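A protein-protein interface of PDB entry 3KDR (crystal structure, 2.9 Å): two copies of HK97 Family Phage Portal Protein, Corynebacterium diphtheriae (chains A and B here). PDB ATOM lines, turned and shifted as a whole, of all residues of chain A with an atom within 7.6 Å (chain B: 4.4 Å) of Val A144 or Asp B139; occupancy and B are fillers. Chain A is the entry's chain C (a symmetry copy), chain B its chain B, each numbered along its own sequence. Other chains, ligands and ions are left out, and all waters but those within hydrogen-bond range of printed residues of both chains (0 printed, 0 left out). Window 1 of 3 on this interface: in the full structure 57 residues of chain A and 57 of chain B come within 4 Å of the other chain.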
ATOM      1  N   ILE A  17      -7.213 -28.963  18.087  1.00  0.00           N
ATOM      2  CA  ILE A  17      -5.797 -29.233  17.767  1.00  0.00           C
ATOM      3  C   ILE A  17      -5.671 -30.580  17.032  1.00  0.00           C
ATOM      4  O   ILE A  17      -5.989 -31.621  17.550  1.00  0.00           O
ATOM      5  CB  ILE A  17      -4.942 -29.283  19.028  1.00  0.00           C
ATOM      6  CG1 ILE A  17      -5.120 -27.991  19.811  1.00  0.00           C
ATOM      7  CG2 ILE A  17      -3.531 -29.507  18.703  1.00  0.00           C
ATOM      8  CD1 ILE A  17      -4.908 -28.145  21.273  1.00  0.00           C
ATOM      9  N   PRO A  18      -5.213 -30.540  15.802  1.00  0.00           N
ATOM     10  CA  PRO A  18      -5.368 -31.727  15.004  1.00  0.00           C
ATOM     11  C   PRO A  18      -4.678 -32.937  15.564  1.00  0.00           C
ATOM     12  O   PRO A  18      -5.189 -34.020  15.456  1.00  0.00           O
ATOM     13  CB  PRO A  18      -4.777 -31.321  13.656  1.00  0.00           C
ATOM     14  CG  PRO A  18      -5.103 -29.871  13.559  1.00  0.00           C
ATOM     15  CD  PRO A  18      -5.027 -29.336  14.977  1.00  0.00           C
ATOM     16  N   THR A 138      -2.193 -25.718  25.127  1.00  0.00           N
ATOM     17  CA  THR A 138      -2.202 -24.321  24.855  1.00  0.00           C
ATOM     18  C   THR A 138      -1.015 -24.010  23.991  1.00  0.00           C
ATOM     19  O   THR A 138      -1.124 -23.406  22.915  1.00  0.00           O
ATOM     20  CB  THR A 138      -2.062 -23.532  26.116  1.00  0.00           C
ATOM     21  OG1 THR A 138      -3.150 -23.847  26.991  1.00  0.00           O
ATOM     22  CG2 THR A 138      -2.054 -22.060  25.820  1.00  0.00           C
ATOM     23  N   ASP A 139       0.130 -24.453  24.452  1.00  0.00           N
ATOM     24  CA  ASP A 139       1.331 -24.301  23.687  1.00  0.00           C
ATOM     25  C   ASP A 139       1.168 -24.845  22.275  1.00  0.00           C
ATOM     26  O   ASP A 139       1.641 -24.256  21.340  1.00  0.00           O
ATOM     27  CB  ASP A 139       2.480 -25.030  24.394  1.00  0.00           C
ATOM     28  CG  ASP A 139       3.800 -25.092  23.529  1.00  0.00           C
ATOM     29  OD1 ASP A 139       4.299 -23.970  23.151  1.00  0.00           O
ATOM     30  OD2 ASP A 139       4.340 -26.241  23.248  1.00  0.00           O
ATOM     31  N   ALA A 140       0.518 -25.982  22.126  1.00  0.00           N
ATOM     32  CA  ALA A 140       0.403 -26.607  20.809  1.00  0.00           C
ATOM     33  C   ALA A 140      -0.426 -25.754  19.889  1.00  0.00           C
ATOM     34  O   ALA A 140      -0.112 -25.619  18.698  1.00  0.00           O
ATOM     35  CB  ALA A 140      -0.198 -27.955  20.902  1.00  0.00           C
ATOM     36  N   ARG A 141      -1.496 -25.183  20.424  1.00  0.00           N
ATOM     37  CA  ARG A 141      -2.367 -24.426  19.600  1.00  0.00           C
ATOM     38  C   ARG A 141      -1.722 -23.104  19.377  1.00  0.00           C
ATOM     39  O   ARG A 141      -1.832 -22.546  18.300  1.00  0.00           O
ATOM     40  CB  ARG A 141      -3.676 -24.250  20.304  1.00  0.00           C
ATOM     41  CG  ARG A 141      -4.756 -23.625  19.454  1.00  0.00           C
ATOM     42  CD  ARG A 141      -5.813 -22.965  20.338  1.00  0.00           C
ATOM     43  NE  ARG A 141      -5.184 -22.163  21.374  1.00  0.00           N
ATOM     44  CZ  ARG A 141      -5.846 -21.691  22.413  1.00  0.00           C
ATOM     45  NH1 ARG A 141      -7.169 -21.947  22.541  1.00  0.00           N
ATOM     46  NH2 ARG A 141      -5.182 -20.954  23.315  1.00  0.00           N
ATOM     47  N   ASN A 142      -1.058 -22.577  20.396  1.00  0.00           N
ATOM     48  CA  ASN A 142      -0.528 -21.209  20.285  1.00  0.00           C
ATOM     49  C   ASN A 142       0.541 -21.078  19.265  1.00  0.00           C
ATOM     50  O   ASN A 142       0.689 -20.066  18.651  1.00  0.00           O
ATOM     51  CB  ASN A 142       0.014 -20.693  21.616  1.00  0.00           C
ATOM     52  CG  ASN A 142      -1.053 -20.038  22.458  1.00  0.00           C
ATOM     53  OD1 ASN A 142      -0.781 -19.577  23.554  1.00  0.00           O
ATOM     54  ND2 ASN A 142      -2.285 -20.020  21.957  1.00  0.00           N
ATOM     55  N   LEU A 143       1.292 -22.145  19.120  1.00  0.00           N
ATOM     56  CA  LEU A 143       2.379 -22.252  18.162  1.00  0.00           C
ATOM     57  C   LEU A 143       1.933 -22.110  16.738  1.00  0.00           C
ATOM     58  O   LEU A 143       2.624 -21.512  15.925  1.00  0.00           O
ATOM     59  CB  LEU A 143       3.027 -23.609  18.286  1.00  0.00           C
ATOM     60  CG  LEU A 143       4.501 -23.480  18.565  1.00  0.00           C
ATOM     61  CD1 LEU A 143       5.024 -24.676  19.282  1.00  0.00           C
ATOM     62  CD2 LEU A 143       5.179 -23.345  17.270  1.00  0.00           C
ATOM     63  N   VAL A 144       0.787 -22.678  16.421  1.00  0.00           N
ATOM     64  CA  VAL A 144       0.273 -22.564  15.065  1.00  0.00           C
ATOM     65  C   VAL A 144      -0.125 -21.115  14.759  1.00  0.00           C
ATOM     66  O   VAL A 144       0.178 -20.586  13.686  1.00  0.00           O
ATOM     67  CB  VAL A 144      -0.864 -23.552  14.797  1.00  0.00           C
ATOM     68  CG1 VAL A 144      -1.356 -23.391  13.384  1.00  0.00           C
ATOM     69  CG2 VAL A 144      -0.347 -24.981  15.027  1.00  0.00           C
ATOM     70  N   ARG A 145      -0.749 -20.458  15.724  1.00  0.00           N
ATOM     71  CA  ARG A 145      -1.207 -19.050  15.548  1.00  0.00           C
ATOM     72  C   ARG A 145      -0.072 -18.026  15.423  1.00  0.00           C
ATOM     73  O   ARG A 145      -0.175 -17.071  14.678  1.00  0.00           O
ATOM     74  CB  ARG A 145      -2.114 -18.640  16.711  1.00  0.00           C
ATOM     75  CG  ARG A 145      -3.390 -19.360  16.681  1.00  0.00           C
ATOM     76  CD  ARG A 145      -4.201 -18.975  17.849  1.00  0.00           C
ATOM     77  NE  ARG A 145      -5.454 -19.719  17.843  1.00  0.00           N
ATOM     78  CZ  ARG A 145      -6.340 -19.662  18.811  1.00  0.00           C
ATOM     79  NH1 ARG A 145      -6.096 -18.911  19.869  1.00  0.00           N
ATOM     80  NH2 ARG A 145      -7.441 -20.383  18.729  1.00  0.00           N
ATOM     81  N   ALA A 146       0.980 -18.242  16.196  1.00  0.00           N
ATOM     82  CA  ALA A 146       2.165 -17.453  16.121  1.00  0.00           C
ATOM     83  C   ALA A 146       2.710 -17.505  14.702  1.00  0.00           C
ATOM     84  O   ALA A 146       3.059 -16.477  14.133  1.00  0.00           O
ATOM     85  CB  ALA A 146       3.200 -17.968  17.126  1.00  0.00           C
ATOM     86  N   ALA A 147       2.766 -18.704  14.131  1.00  0.00           N
ATOM     87  CA  ALA A 147       3.329 -18.921  12.803  1.00  0.00           C
ATOM     88  C   ALA A 147       2.487 -18.291  11.721  1.00  0.00           C
ATOM     89  O   ALA A 147       3.000 -17.942  10.648  1.00  0.00           O
ATOM     90  CB  ALA A 147       3.402 -20.370  12.540  1.00  0.00           C
ATOM     91  N   ALA A 148       1.174 -18.210  11.978  1.00  0.00           N
ATOM     92  CA  ALA A 148       0.265 -17.470  11.102  1.00  0.00           C
ATOM     93  C   ALA A 148       0.531 -15.950  11.170  1.00  0.00           C
ATOM     94  O   ALA A 148       0.662 -15.314  10.143  1.00  0.00           O
ATOM     95  CB  ALA A 148      -1.146 -17.770  11.459  1.00  0.00           C
ATOM     96  N   ARG A 149       0.599 -15.379  12.375  1.00  0.00           N
ATOM     97  CA  ARG A 149       0.989 -13.976  12.555  1.00  0.00           C
ATOM     98  C   ARG A 149       2.339 -13.754  11.959  1.00  0.00           C
ATOM     99  O   ARG A 149       2.554 -12.850  11.138  1.00  0.00           O
ATOM    100  CB  ARG A 149       1.193 -13.607  14.028  1.00  0.00           C
ATOM    101  CG  ARG A 149      -0.052 -13.344  14.864  1.00  0.00           C
ATOM    102  CD  ARG A 149       0.312 -13.260  16.353  1.00  0.00           C
ATOM    103  NE  ARG A 149      -0.175 -14.423  17.109  1.00  0.00           N
ATOM    104  CZ  ARG A 149       0.037 -14.611  18.416  1.00  0.00           C
ATOM    105  NH1 ARG A 149       0.738 -13.699  19.104  1.00  0.00           N
ATOM    106  NH2 ARG A 149      -0.433 -15.703  19.039  1.00  0.00           N
ATOM    107  N   VAL A 150       3.261 -14.587  12.413  1.00  0.00           N
ATOM    108  CA  VAL A 150       4.645 -14.326  12.210  1.00  0.00           C
ATOM    109  C   VAL A 150       5.032 -14.455  10.792  1.00  0.00           C
ATOM    110  O   VAL A 150       5.921 -13.789  10.359  1.00  0.00           O
ATOM    111  CB  VAL A 150       5.522 -15.262  13.012  1.00  0.00           C
ATOM    112  CG1 VAL A 150       6.954 -15.135  12.592  1.00  0.00           C
ATOM    113  CG2 VAL A 150       5.414 -14.928  14.420  1.00  0.00           C
ATOM    114  N   LEU A 211      10.005 -21.667  15.833  1.00  0.00           N
ATOM    115  CA  LEU A 211       8.639 -21.929  15.529  1.00  0.00           C
ATOM    116  C   LEU A 211       8.477 -23.211  14.691  1.00  0.00           C
ATOM    117  O   LEU A 211       7.475 -23.923  14.803  1.00  0.00           O
ATOM    118  CB  LEU A 211       8.065 -20.724  14.787  1.00  0.00           C
ATOM    119  CG  LEU A 211       7.797 -19.474  15.633  1.00  0.00           C
ATOM    120  CD1 LEU A 211       7.215 -18.334  14.719  1.00  0.00           C
ATOM    121  CD2 LEU A 211       6.856 -19.747  16.790  1.00  0.00           C
ATOM    122  N   ARG A 215       6.731 -26.595  16.454  1.00  0.00           N
ATOM    123  CA  ARG A 215       5.517 -27.187  15.988  1.00  0.00           C
ATOM    124  C   ARG A 215       5.601 -28.669  16.056  1.00  0.00           C
ATOM    125  O   ARG A 215       4.665 -29.321  16.475  1.00  0.00           O
ATOM    126  CB  ARG A 215       5.239 -26.831  14.542  1.00  0.00           C
ATOM    127  CG  ARG A 215       3.759 -26.607  14.302  1.00  0.00           C
ATOM    128  CD  ARG A 215       3.441 -26.414  12.866  1.00  0.00           C
ATOM    129  NE  ARG A 215       2.026 -26.597  12.533  1.00  0.00           N
ATOM    130  CZ  ARG A 215       1.432 -25.971  11.524  1.00  0.00           C
ATOM    131  NH1 ARG A 215       2.055 -25.074  10.777  1.00  0.00           N
ATOM    132  NH2 ARG A 215       0.198 -26.221  11.243  1.00  0.00           N
ATOM    133  N   ALA A 218       5.680 -29.790  19.535  1.00  0.00           N
ATOM    134  CA  ALA A 218       4.385 -29.695  20.177  1.00  0.00           C
ATOM    135  C   ALA A 218       3.634 -30.982  19.878  1.00  0.00           C
ATOM    136  O   ALA A 218       3.017 -31.588  20.763  1.00  0.00           O
ATOM    137  CB  ALA A 218       3.625 -28.466  19.721  1.00  0.00           C
ATOM    138  N   GLU B 135     -10.411 -23.936  12.429  1.00  0.00           N
ATOM    139  CA  GLU B 135      -9.140 -23.255  12.551  1.00  0.00           C
ATOM    140  C   GLU B 135      -8.042 -23.804  11.605  1.00  0.00           C
ATOM    141  O   GLU B 135      -7.314 -23.042  10.963  1.00  0.00           O
ATOM    142  CB  GLU B 135      -8.653 -23.365  13.995  1.00  0.00           C
ATOM    143  CG  GLU B 135      -8.460 -22.049  14.683  1.00  0.00           C
ATOM    144  CD  GLU B 135      -7.515 -22.138  15.894  1.00  0.00           C
ATOM    145  OE1 GLU B 135      -6.334 -21.644  15.814  1.00  0.00           O
ATOM    146  OE2 GLU B 135      -7.974 -22.700  16.931  1.00  0.00           O
ATOM    147  N   THR B 136      -7.882 -25.114  11.548  1.00  0.00           N
ATOM    148  CA  THR B 136      -6.771 -25.708  10.804  1.00  0.00           C
ATOM    149  C   THR B 136      -7.013 -25.538   9.351  1.00  0.00           C
ATOM    150  O   THR B 136      -6.068 -25.276   8.611  1.00  0.00           O
ATOM    151  CB  THR B 136      -6.596 -27.235  10.979  1.00  0.00           C
ATOM    152  OG1 THR B 136      -7.348 -27.688  12.106  1.00  0.00           O
ATOM    153  CG2 THR B 136      -5.132 -27.571  11.154  1.00  0.00           C
ATOM    154  N   PHE B 137      -8.262 -25.733   8.938  1.00  0.00           N
ATOM    155  CA  PHE B 137      -8.618 -25.491   7.563  1.00  0.00           C
ATOM    156  C   PHE B 137      -8.357 -24.029   7.217  1.00  0.00           C
ATOM    157  O   PHE B 137      -7.820 -23.733   6.176  1.00  0.00           O
ATOM    158  CB  PHE B 137     -10.086 -25.797   7.300  1.00  0.00           C
ATOM    159  CG  PHE B 137     -10.445 -27.254   7.370  1.00  0.00           C
ATOM    160  CD1 PHE B 137      -9.496 -28.234   7.382  1.00  0.00           C
ATOM    161  CD2 PHE B 137     -11.764 -27.644   7.388  1.00  0.00           C
ATOM    162  CE1 PHE B 137      -9.842 -29.553   7.423  1.00  0.00           C
ATOM    163  CE2 PHE B 137     -12.104 -28.974   7.441  1.00  0.00           C
ATOM    164  CZ  PHE B 137     -11.126 -29.915   7.455  1.00  0.00           C
ATOM    165  N   THR B 138      -8.744 -23.115   8.087  1.00  0.00           N
ATOM    166  CA  THR B 138      -8.520 -21.718   7.818  1.00  0.00           C
ATOM    167  C   THR B 138      -7.024 -21.441   7.633  1.00  0.00           C
ATOM    168  O   THR B 138      -6.598 -20.712   6.711  1.00  0.00           O
ATOM    169  CB  THR B 138      -9.051 -20.826   8.967  1.00  0.00           C
ATOM    170  OG1 THR B 138     -10.465 -20.941   9.053  1.00  0.00           O
ATOM    171  CG2 THR B 138      -8.688 -19.391   8.727  1.00  0.00           C
ATOM    172  N   ASP B 139      -6.223 -22.028   8.510  1.00  0.00           N
ATOM    173  CA  ASP B 139      -4.786 -21.851   8.378  1.00  0.00           C
ATOM    174  C   ASP B 139      -4.225 -22.437   7.095  1.00  0.00           C
ATOM    175  O   ASP B 139      -3.334 -21.852   6.495  1.00  0.00           O
ATOM    176  CB  ASP B 139      -4.031 -22.393   9.590  1.00  0.00           C
ATOM    177  CG  ASP B 139      -4.144 -21.454  10.828  1.00  0.00           C
ATOM    178  OD1 ASP B 139      -4.831 -20.393  10.779  1.00  0.00           O
ATOM    179  OD2 ASP B 139      -3.528 -21.769  11.880  1.00  0.00           O
ATOM    180  N   ALA B 140      -4.747 -23.580   6.670  1.00  0.00           N
ATOM    181  CA  ALA B 140      -4.170 -24.270   5.542  1.00  0.00           C
ATOM    182  C   ALA B 140      -4.454 -23.492   4.295  1.00  0.00           C
ATOM    183  O   ALA B 140      -3.632 -23.429   3.387  1.00  0.00           O
ATOM    184  CB  ALA B 140      -4.744 -25.623   5.406  1.00  0.00           C
ATOM    185  N   ARG B 141      -5.635 -22.902   4.236  1.00  0.00           N
ATOM    186  CA  ARG B 141      -6.023 -22.143   3.091  1.00  0.00           C
ATOM    187  C   ARG B 141      -5.220 -20.886   3.074  1.00  0.00           C
ATOM    188  O   ARG B 141      -4.690 -20.513   2.018  1.00  0.00           O
ATOM    189  CB  ARG B 141      -7.499 -21.821   3.233  1.00  0.00           C
ATOM    190  CG  ARG B 141      -8.235 -21.350   1.990  1.00  0.00           C
ATOM    191  CD  ARG B 141      -8.641 -19.941   2.159  1.00  0.00           C
ATOM    192  NE  ARG B 141     -10.009 -19.789   2.640  1.00  0.00           N
ATOM    193  CZ  ARG B 141     -10.377 -19.009   3.654  1.00  0.00           C
ATOM    194  NH1 ARG B 141      -9.483 -18.306   4.362  1.00  0.00           N
ATOM    195  NH2 ARG B 141     -11.664 -18.959   3.983  1.00  0.00           N
ATOM    196  N   ASN B 142      -5.137 -20.220   4.237  1.00  0.00           N
ATOM    197  CA  ASN B 142      -4.514 -18.894   4.298  1.00  0.00           C
ATOM    198  C   ASN B 142      -3.066 -18.943   3.929  1.00  0.00           C
ATOM    199  O   ASN B 142      -2.498 -17.973   3.395  1.00  0.00           O
ATOM    200  CB  ASN B 142      -4.597 -18.300   5.694  1.00  0.00           C
ATOM    201  CG  ASN B 142      -5.909 -17.630   5.946  1.00  0.00           C
ATOM    202  OD1 ASN B 142      -6.651 -17.351   5.015  1.00  0.00           O
ATOM    203  ND2 ASN B 142      -6.223 -17.391   7.209  1.00  0.00           N
ATOM    204  N   LEU B 143      -2.455 -20.078   4.239  1.00  0.00           N
ATOM    205  CA  LEU B 143      -1.020 -20.210   4.118  1.00  0.00           C
ATOM    206  C   LEU B 143      -0.644 -20.156   2.679  1.00  0.00           C
ATOM    207  O   LEU B 143       0.345 -19.535   2.315  1.00  0.00           O
ATOM    208  CB  LEU B 143      -0.567 -21.520   4.713  1.00  0.00           C
ATOM    209  CG  LEU B 143       0.833 -21.499   5.259  1.00  0.00           C
ATOM    210  CD1 LEU B 143       0.759 -22.068   6.631  1.00  0.00           C
ATOM    211  CD2 LEU B 143       1.695 -22.314   4.353  1.00  0.00           C
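OE1 of Glu B135 is in salt-bridge range of NE of Arg A145, at 2.9 Å.
Among the printed residues, merely in contact across the chains: Val A144 with Asp B139 (3.1 Å) and Pro A18 with Thr B136 (3.3 Å).
Val A144 touches just one residue of chain B: Asp B139. Asp B139 touches just one residue of chain A: Val A144 (3.1 Å). Printed residues of chain A within 4 Å of Glu B135: Arg A145 (2.9 Å). Of the printed residues of chain B, Arg A145 touches Glu B135. Of the printed residues of chain B, Pro A18 touches Thr B136 (3.3 Å). Of the printed residues of chain A, Thr B136 touches Pro A18 (3.3 Å). Phe B137 touches none of the printed residues of chain A. Thr A138 touches none of the printed residues of chain B. The nearest printed residue of chain B that does not touch Pro A18 is Phe B137 (7.0 Å).
Of the 9 printed residues of chain B, 3 touch a printed residue of chain A. Printed residues of chain B that touch a printed residue of chain A: Glu B135, Thr B136 and Asp B139. Printed residues of chain A that touch a printed residue of chain B: Pro A18, Val A144 and Arg A145. Hydrophobic or aromatic side chains of chain A within 4 Å of the printed part of chain B: Pro A18 and Val A144.
6 positions are printed for both chains. Of the 3 pairs that touch across the chains among the printed residues, none has its exchanged pair printed and touching as well.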
